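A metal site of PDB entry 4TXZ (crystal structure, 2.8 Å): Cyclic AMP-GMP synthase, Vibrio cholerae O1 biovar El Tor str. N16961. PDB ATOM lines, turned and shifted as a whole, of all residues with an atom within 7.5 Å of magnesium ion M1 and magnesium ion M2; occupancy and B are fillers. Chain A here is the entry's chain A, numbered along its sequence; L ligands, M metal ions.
The backbone NH of Ser 114 lies within hydrogen-bond range of an oxygen (O5) of the ligand, at 3.4 Å. An oxygen (O1) of the ligand sits at hydrogen-bond distance from the side-chain hydroxyl of Ser 114, 2.9 Å away. The backbone NH of Gly 113 lies within hydrogen-bond range of an oxygen (O11) of the ligand, at 3.3 Å. The side-chain amide nitrogen (NE2) of Gln 112 lies within hydrogen-bond range of an oxygen (O10) of the ligand (3.4 Å). OH of Tyr 117 is in hydrogen-bond range of O5 of the ligand (2.7 Å). The side-chain amino group of Lys 287 lies within salt-bridge range of an oxygen (O1) of the ligand, at 2.8 Å.
The backbone NH (N) of Gln 112 sits at hydrogen-bond distance from the backbone carbonyl oxygen (O) of Asp 133, 2.9 Å away. OD1 of Asp 193 lies within salt-bridge range of NE of Arg 182. The backbone NH (N) of Asp 193 lies within hydrogen-bond range of the backbone carbonyl oxygen (O) of Ile 132. N of Asp 134 sits at hydrogen-bond distance from O of Asp 193, 2.9 Å away. NE2 of His 191 lies close to OD1 of Asp 131 (2.8 Å). O of Ser 114 sits at hydrogen-bond distance from N of Thr 119 (2.9 Å).
Gly 113 touches magnesium ion M2 (CA to MG, 3.8 Å). Ser 114 touches magnesium ion M2 (OG to MG, 3.1 Å).
Magnesium ion M1 is bound by the side-chain carboxylate of Asp 133 (2.1 Å), the side-chain carboxylate of Asp 193 (2.2 Å) and the side-chain carboxylate of Asp 131 (2.3 Å). Slightly farther from magnesium ion M1 lies OD2 of Asp 131 (2.8 Å).
Magnesium ion M2 is bound by OD2 of Asp 133 (2.1 Å), O6 of the ligand (2.1 Å) and OD2 of Asp 131 (2.3 Å). Slightly farther from magnesium ion M2 lies an oxygen (O2) of the ligand (2.8 Å).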
ATOM      1  N   THR A 111      -6.851  24.083  25.128  1.00  0.00           N
ATOM      2  CA  THR A 111      -7.256  22.717  25.447  1.00  0.00           C
ATOM      3  C   THR A 111      -7.905  22.040  24.234  1.00  0.00           C
ATOM      4  O   THR A 111      -8.594  22.683  23.448  1.00  0.00           O
ATOM      5  CB  THR A 111      -8.235  22.704  26.645  1.00  0.00           C
ATOM      6  OG1 THR A 111      -7.632  23.373  27.761  1.00  0.00           O
ATOM      7  CG2 THR A 111      -8.605  21.278  27.042  1.00  0.00           C
ATOM      8  N   GLN A 112      -7.655  20.742  24.094  1.00  0.00           N
ATOM      9  CA  GLN A 112      -8.223  19.932  23.034  1.00  0.00           C
ATOM     10  C   GLN A 112      -8.776  18.643  23.620  1.00  0.00           C
ATOM     11  O   GLN A 112      -8.586  18.361  24.805  1.00  0.00           O
ATOM     12  CB  GLN A 112      -7.183  19.613  21.969  1.00  0.00           C
ATOM     13  CG  GLN A 112      -6.158  18.578  22.429  1.00  0.00           C
ATOM     14  CD  GLN A 112      -4.819  18.717  21.715  1.00  0.00           C
ATOM     15  OE1 GLN A 112      -4.244  19.796  21.652  1.00  0.00           O
ATOM     16  NE2 GLN A 112      -4.327  17.604  21.178  1.00  0.00           N
ATOM     17  N   GLY A 113      -9.468  17.868  22.796  1.00  0.00           N
ATOM     18  CA  GLY A 113      -9.990  16.583  23.232  1.00  0.00           C
ATOM     19  C   GLY A 113     -11.343  16.666  23.894  1.00  0.00           C
ATOM     20  O   GLY A 113     -12.071  17.641  23.740  1.00  0.00           O
ATOM     21  N   SER A 114     -11.672  15.612  24.642  1.00  0.00           N
ATOM     22  CA  SER A 114     -12.970  15.477  25.297  1.00  0.00           C
ATOM     23  C   SER A 114     -13.340  16.668  26.182  1.00  0.00           C
ATOM     24  O   SER A 114     -14.495  17.098  26.197  1.00  0.00           O
ATOM     25  CB  SER A 114     -12.990  14.184  26.133  1.00  0.00           C
ATOM     26  OG  SER A 114     -11.730  13.941  26.731  1.00  0.00           O
ATOM     27  N   PHE A 115     -12.374  17.195  26.918  1.00  0.00           N
ATOM     28  CA  PHE A 115     -12.634  18.320  27.815  1.00  0.00           C
ATOM     29  C   PHE A 115     -12.961  19.597  27.037  1.00  0.00           C
ATOM     30  O   PHE A 115     -13.606  20.500  27.569  1.00  0.00           O
ATOM     31  CB  PHE A 115     -11.433  18.563  28.729  1.00  0.00           C
ATOM     32  CG  PHE A 115     -11.767  19.360  29.970  1.00  0.00           C
ATOM     33  CD1 PHE A 115     -12.427  18.769  31.026  1.00  0.00           C
ATOM     34  CD2 PHE A 115     -11.426  20.698  30.055  1.00  0.00           C
ATOM     35  CE1 PHE A 115     -12.745  19.496  32.155  1.00  0.00           C
ATOM     36  CE2 PHE A 115     -11.741  21.434  31.187  1.00  0.00           C
ATOM     37  CZ  PHE A 115     -12.404  20.834  32.240  1.00  0.00           C
ATOM     38  N   GLN A 116     -12.528  19.656  25.783  1.00  0.00           N
ATOM     39  CA  GLN A 116     -12.794  20.829  24.948  1.00  0.00           C
ATOM     40  C   GLN A 116     -14.176  20.778  24.298  1.00  0.00           C
ATOM     41  O   GLN A 116     -14.923  21.761  24.349  1.00  0.00           O
ATOM     42  CB  GLN A 116     -11.721  20.967  23.878  1.00  0.00           C
ATOM     43  CG  GLN A 116     -11.787  22.275  23.092  1.00  0.00           C
ATOM     44  CD  GLN A 116     -11.790  23.504  24.002  1.00  0.00           C
ATOM     45  OE1 GLN A 116     -11.042  23.568  24.973  1.00  0.00           O
ATOM     46  NE2 GLN A 116     -12.626  24.473  23.675  1.00  0.00           N
ATOM     47  N   TYR A 117     -14.526  19.645  23.690  1.00  0.00           N
ATOM     48  CA  TYR A 117     -15.838  19.520  23.052  1.00  0.00           C
ATOM     49  C   TYR A 117     -16.813  18.684  23.873  1.00  0.00           C
ATOM     50  O   TYR A 117     -17.757  18.112  23.320  1.00  0.00           O
ATOM     51  CB  TYR A 117     -15.713  18.953  21.637  1.00  0.00           C
ATOM     52  CG  TYR A 117     -14.602  17.956  21.396  1.00  0.00           C
ATOM     53  CD1 TYR A 117     -14.679  16.655  21.874  1.00  0.00           C
ATOM     54  CD2 TYR A 117     -13.484  18.307  20.648  1.00  0.00           C
ATOM     55  CE1 TYR A 117     -13.671  15.747  21.643  1.00  0.00           C
ATOM     56  CE2 TYR A 117     -12.468  17.399  20.410  1.00  0.00           C
ATOM     57  CZ  TYR A 117     -12.568  16.121  20.907  1.00  0.00           C
ATOM     58  OH  TYR A 117     -11.552  15.213  20.669  1.00  0.00           O
ATOM     59  N   THR A 119     -16.980  15.730  25.864  1.00  0.00           N
ATOM     60  CA  THR A 119     -17.250  14.310  25.715  1.00  0.00           C
ATOM     61  C   THR A 119     -16.444  13.496  26.730  1.00  0.00           C
ATOM     62  O   THR A 119     -16.205  12.308  26.537  1.00  0.00           O
ATOM     63  CB  THR A 119     -16.933  13.796  24.304  1.00  0.00           C
ATOM     64  OG1 THR A 119     -15.651  14.280  23.889  1.00  0.00           O
ATOM     65  CG2 THR A 119     -17.983  14.279  23.313  1.00  0.00           C
ATOM     66  N   LEU A 120     -16.036  14.160  27.802  1.00  0.00           N
ATOM     67  CA  LEU A 120     -15.246  13.510  28.845  1.00  0.00           C
ATOM     68  C   LEU A 120     -16.124  12.639  29.736  1.00  0.00           C
ATOM     69  O   LEU A 120     -16.988  13.151  30.449  1.00  0.00           O
ATOM     70  CB  LEU A 120     -14.502  14.548  29.688  1.00  0.00           C
ATOM     71  CG  LEU A 120     -13.055  14.238  30.079  1.00  0.00           C
ATOM     72  CD1 LEU A 120     -12.730  14.853  31.430  1.00  0.00           C
ATOM     73  CD2 LEU A 120     -12.756  12.744  30.078  1.00  0.00           C
ATOM     74  N   MET A 130      -9.356  10.030  33.814  1.00  0.00           N
ATOM     75  CA  MET A 130      -9.793  11.195  33.057  1.00  0.00           C
ATOM     76  C   MET A 130      -8.616  11.790  32.310  1.00  0.00           C
ATOM     77  O   MET A 130      -7.555  12.005  32.879  1.00  0.00           O
ATOM     78  CB  MET A 130     -10.421  12.244  33.978  1.00  0.00           C
ATOM     79  CG  MET A 130     -11.674  11.788  34.686  1.00  0.00           C
ATOM     80  SD  MET A 130     -12.064  12.838  36.099  1.00  0.00           S
ATOM     81  CE  MET A 130     -13.486  11.984  36.786  1.00  0.00           C
ATOM     82  N   ASP A 131      -8.829  12.058  31.023  1.00  0.00           N
ATOM     83  CA  ASP A 131      -7.744  12.558  30.193  1.00  0.00           C
ATOM     84  C   ASP A 131      -7.986  14.006  29.821  1.00  0.00           C
ATOM     85  O   ASP A 131      -8.964  14.330  29.144  1.00  0.00           O
ATOM     86  CB  ASP A 131      -7.614  11.695  28.935  1.00  0.00           C
ATOM     87  CG  ASP A 131      -6.776  12.360  27.864  1.00  0.00           C
ATOM     88  OD1 ASP A 131      -5.589  12.639  28.127  1.00  0.00           O
ATOM     89  OD2 ASP A 131      -7.299  12.604  26.756  1.00  0.00           O
ATOM     90  N   ILE A 132      -7.108  14.898  30.281  1.00  0.00           N
ATOM     91  CA  ILE A 132      -7.231  16.296  29.867  1.00  0.00           C
ATOM     92  C   ILE A 132      -6.020  16.753  29.065  1.00  0.00           C
ATOM     93  O   ILE A 132      -4.901  16.791  29.564  1.00  0.00           O
ATOM     94  CB  ILE A 132      -7.477  17.227  31.076  1.00  0.00           C
ATOM     95  CG1 ILE A 132      -7.436  18.698  30.630  1.00  0.00           C
ATOM     96  CG2 ILE A 132      -6.478  16.964  32.200  1.00  0.00           C
ATOM     97  CD1 ILE A 132      -8.046  19.661  31.627  1.00  0.00           C
ATOM     98  N   ASP A 133      -6.250  17.098  27.796  1.00  0.00           N
ATOM     99  CA  ASP A 133      -5.167  17.505  26.912  1.00  0.00           C
ATOM    100  C   ASP A 133      -5.096  19.027  26.758  1.00  0.00           C
ATOM    101  O   ASP A 133      -5.944  19.625  26.115  1.00  0.00           O
ATOM    102  CB  ASP A 133      -5.330  16.861  25.539  1.00  0.00           C
ATOM    103  CG  ASP A 133      -5.741  15.410  25.612  1.00  0.00           C
ATOM    104  OD1 ASP A 133      -4.876  14.559  25.916  1.00  0.00           O
ATOM    105  OD2 ASP A 133      -6.926  15.117  25.353  1.00  0.00           O
ATOM    106  N   ASP A 134      -4.078  19.639  27.346  1.00  0.00           N
ATOM    107  CA  ASP A 134      -3.882  21.075  27.253  1.00  0.00           C
ATOM    108  C   ASP A 134      -2.629  21.382  26.454  1.00  0.00           C
ATOM    109  O   ASP A 134      -1.511  21.233  26.953  1.00  0.00           O
ATOM    110  CB  ASP A 134      -3.800  21.709  28.642  1.00  0.00           C
ATOM    111  CG  ASP A 134      -4.088  23.192  28.627  1.00  0.00           C
ATOM    112  OD1 ASP A 134      -4.927  23.633  27.809  1.00  0.00           O
ATOM    113  OD2 ASP A 134      -3.460  23.932  29.425  1.00  0.00           O
ATOM    114  N   CYS A 180       3.682  14.337  23.366  1.00  0.00           N
ATOM    115  CA  CYS A 180       3.397  15.177  24.523  1.00  0.00           C
ATOM    116  C   CYS A 180       4.107  14.744  25.805  1.00  0.00           C
ATOM    117  O   CYS A 180       4.584  13.618  25.914  1.00  0.00           O
ATOM    118  CB  CYS A 180       1.888  15.185  24.795  1.00  0.00           C
ATOM    119  SG  CYS A 180       1.242  13.630  25.451  1.00  0.00           S
ATOM    120  N   ARG A 182       3.512  14.223  29.957  1.00  0.00           N
ATOM    121  CA  ARG A 182       2.317  13.866  30.707  1.00  0.00           C
ATOM    122  C   ARG A 182       2.521  13.884  32.219  1.00  0.00           C
ATOM    123  O   ARG A 182       3.564  13.451  32.719  1.00  0.00           O
ATOM    124  CB  ARG A 182       1.816  12.488  30.271  1.00  0.00           C
ATOM    125  CG  ARG A 182       0.769  11.876  31.201  1.00  0.00           C
ATOM    126  CD  ARG A 182       0.309  10.503  30.735  1.00  0.00           C
ATOM    127  NE  ARG A 182      -0.523  10.595  29.542  1.00  0.00           N
ATOM    128  CZ  ARG A 182      -1.099   9.547  28.956  1.00  0.00           C
ATOM    129  NH1 ARG A 182      -0.934   8.332  29.448  1.00  0.00           N
ATOM    130  NH2 ARG A 182      -1.846   9.719  27.871  1.00  0.00           N
ATOM    131  N   HIS A 191      -5.155  12.276  34.476  1.00  0.00           N
ATOM    132  CA  HIS A 191      -3.864  12.625  33.886  1.00  0.00           C
ATOM    133  C   HIS A 191      -4.006  13.766  32.875  1.00  0.00           C
ATOM    134  O   HIS A 191      -5.038  13.902  32.184  1.00  0.00           O
ATOM    135  CB  HIS A 191      -3.205  11.402  33.232  1.00  0.00           C
ATOM    136  CG  HIS A 191      -3.828  10.988  31.931  1.00  0.00           C
ATOM    137  ND1 HIS A 191      -4.641   9.880  31.828  1.00  0.00           N
ATOM    138  CD2 HIS A 191      -3.721  11.494  30.686  1.00  0.00           C
ATOM    139  CE1 HIS A 191      -5.028   9.744  30.577  1.00  0.00           C
ATOM    140  NE2 HIS A 191      -4.483  10.712  29.858  1.00  0.00           N
ATOM    141  N   ILE A 192      -2.962  14.583  32.798  1.00  0.00           N
ATOM    142  CA  ILE A 192      -2.955  15.730  31.913  1.00  0.00           C
ATOM    143  C   ILE A 192      -1.838  15.604  30.888  1.00  0.00           C
ATOM    144  O   ILE A 192      -0.664  15.408  31.228  1.00  0.00           O
ATOM    145  CB  ILE A 192      -2.826  17.060  32.706  1.00  0.00           C
ATOM    146  CG1 ILE A 192      -2.748  18.250  31.746  1.00  0.00           C
ATOM    147  CG2 ILE A 192      -1.634  17.035  33.633  1.00  0.00           C
ATOM    148  CD1 ILE A 192      -3.074  19.579  32.393  1.00  0.00           C
ATOM    149  N   ASP A 193      -2.242  15.665  29.629  1.00  0.00           N
ATOM    150  CA  ASP A 193      -1.316  15.603  28.514  1.00  0.00           C
ATOM    151  C   ASP A 193      -1.009  17.013  28.030  1.00  0.00           C
ATOM    152  O   ASP A 193      -1.913  17.838  27.884  1.00  0.00           O
ATOM    153  CB  ASP A 193      -1.883  14.765  27.365  1.00  0.00           C
ATOM    154  CG  ASP A 193      -1.943  13.293  27.696  1.00  0.00           C
ATOM    155  OD1 ASP A 193      -1.118  12.836  28.515  1.00  0.00           O
ATOM    156  OD2 ASP A 193      -2.810  12.584  27.139  1.00  0.00           O
ATOM    157  N   VAL A 194       0.260  17.280  27.791  1.00  0.00           N
ATOM    158  CA  VAL A 194       0.704  18.568  27.293  1.00  0.00           C
ATOM    159  C   VAL A 194       1.439  18.359  25.986  1.00  0.00           C
ATOM    160  O   VAL A 194       2.657  18.102  25.982  1.00  0.00           O
ATOM    161  CB  VAL A 194       1.605  19.297  28.304  1.00  0.00           C
ATOM    162  CG1 VAL A 194       1.999  20.670  27.770  1.00  0.00           C
ATOM    163  CG2 VAL A 194       0.901  19.430  29.639  1.00  0.00           C
ATOM    164  N   PRO A 195       0.703  18.393  24.865  1.00  0.00           N
ATOM    165  CA  PRO A 195       1.310  18.425  23.539  1.00  0.00           C
ATOM    166  C   PRO A 195       1.807  19.822  23.263  1.00  0.00           C
ATOM    167  O   PRO A 195       1.296  20.786  23.837  1.00  0.00           O
ATOM    168  CB  PRO A 195       0.141  18.047  22.630  1.00  0.00           C
ATOM    169  CG  PRO A 195      -1.043  18.610  23.335  1.00  0.00           C
ATOM    170  CD  PRO A 195      -0.772  18.314  24.786  1.00  0.00           C
ATOM    171  N   LYS A 287     -18.243   5.592  23.773  1.00  0.00           N
ATOM    172  CA  LYS A 287     -16.984   5.626  24.512  1.00  0.00           C
ATOM    173  C   LYS A 287     -17.109   4.832  25.810  1.00  0.00           C
ATOM    174  O   LYS A 287     -16.163   4.174  26.251  1.00  0.00           O
ATOM    175  CB  LYS A 287     -16.568   7.067  24.813  1.00  0.00           C
ATOM    176  CG  LYS A 287     -15.762   7.722  23.706  1.00  0.00           C
ATOM    177  CD  LYS A 287     -15.688   9.228  23.910  1.00  0.00           C
ATOM    178  CE  LYS A 287     -14.856   9.567  25.139  1.00  0.00           C
ATOM    179  NZ  LYS A 287     -14.562  11.024  25.250  1.00  0.00           N
HETATM  180  P1  LIG L   1     -10.783  10.744  25.508  1.00  0.00           P
HETATM  181  O1  LIG L   1     -11.986  11.109  26.334  1.00  0.00           O
HETATM  182  O2  LIG L   1      -9.579  11.501  25.991  1.00  0.00           O
HETATM  183  O3  LIG L   1     -10.520   9.245  25.633  1.00  0.00           O
HETATM  184  O4  LIG L   1     -11.037  11.098  23.964  1.00  0.00           O
HETATM  185  P2  LIG L   1     -10.303  12.307  23.182  1.00  0.00           P
HETATM  186  O5  LIG L   1     -11.305  13.079  22.342  1.00  0.00           O
HETATM  187  O6  LIG L   1      -9.673  13.259  24.179  1.00  0.00           O
HETATM  188  C1  LIG L   1      -9.045  11.561  22.134  1.00  0.00           C
HETATM  189  P3  LIG L   1      -7.296  11.850  22.604  1.00  0.00           P
HETATM  190  O7  LIG L   1      -6.528  10.578  22.359  1.00  0.00           O
HETATM  191  O8  LIG L   1      -7.176  12.228  24.091  1.00  0.00           O
HETATM  192  O9  LIG L   1      -6.686  13.032  21.664  1.00  0.00           O
HETATM  193  C2  LIG L   1      -7.047  14.391  21.946  1.00  0.00           C
HETATM  194  C3  LIG L   1      -6.718  15.197  20.762  1.00  0.00           C
HETATM  195  O10 LIG L   1      -5.545  14.620  20.044  1.00  0.00           O
HETATM  196  C4  LIG L   1      -7.816  15.121  19.767  1.00  0.00           C
HETATM  197  O11 LIG L   1      -8.806  16.124  20.027  1.00  0.00           O
HETATM  198  C5  LIG L   1      -7.133  15.386  18.493  1.00  0.00           C
HETATM  199  O12 LIG L   1      -7.023  16.821  18.254  1.00  0.00           O
HETATM  200  C6  LIG L   1      -5.814  14.806  18.623  1.00  0.00           C
HETATM  201  N1  LIG L   1      -5.768  13.551  17.919  1.00  0.00           N
HETATM  202  C7  LIG L   1      -5.789  12.328  18.471  1.00  0.00           C
HETATM  203  N2  LIG L   1      -5.736  11.412  17.498  1.00  0.00           N
HETATM  204  C8  LIG L   1      -5.675  12.059  16.278  1.00  0.00           C
HETATM  205  C9  LIG L   1      -5.612  11.621  14.948  1.00  0.00           C
HETATM  206  O13 LIG L   1      -5.587  10.418  14.692  1.00  0.00           O
HETATM  207  N3  LIG L   1      -5.560  12.515  13.970  1.00  0.00           N
HETATM  208  C10 LIG L   1      -5.584  13.827  14.264  1.00  0.00           C
HETATM  209  N4  LIG L   1      -5.537  14.762  13.201  1.00  0.00           N
HETATM  210  N5  LIG L   1      -5.652  14.267  15.527  1.00  0.00           N
HETATM  211  C11 LIG L   1      -5.696  13.397  16.557  1.00  0.00           C
HETATM  212 MG    MG M   1      -4.647  12.495  26.009  1.00  0.00          MG
HETATM  213 MG    MG M   2      -8.756  14.182  25.880  1.00  0.00          MG
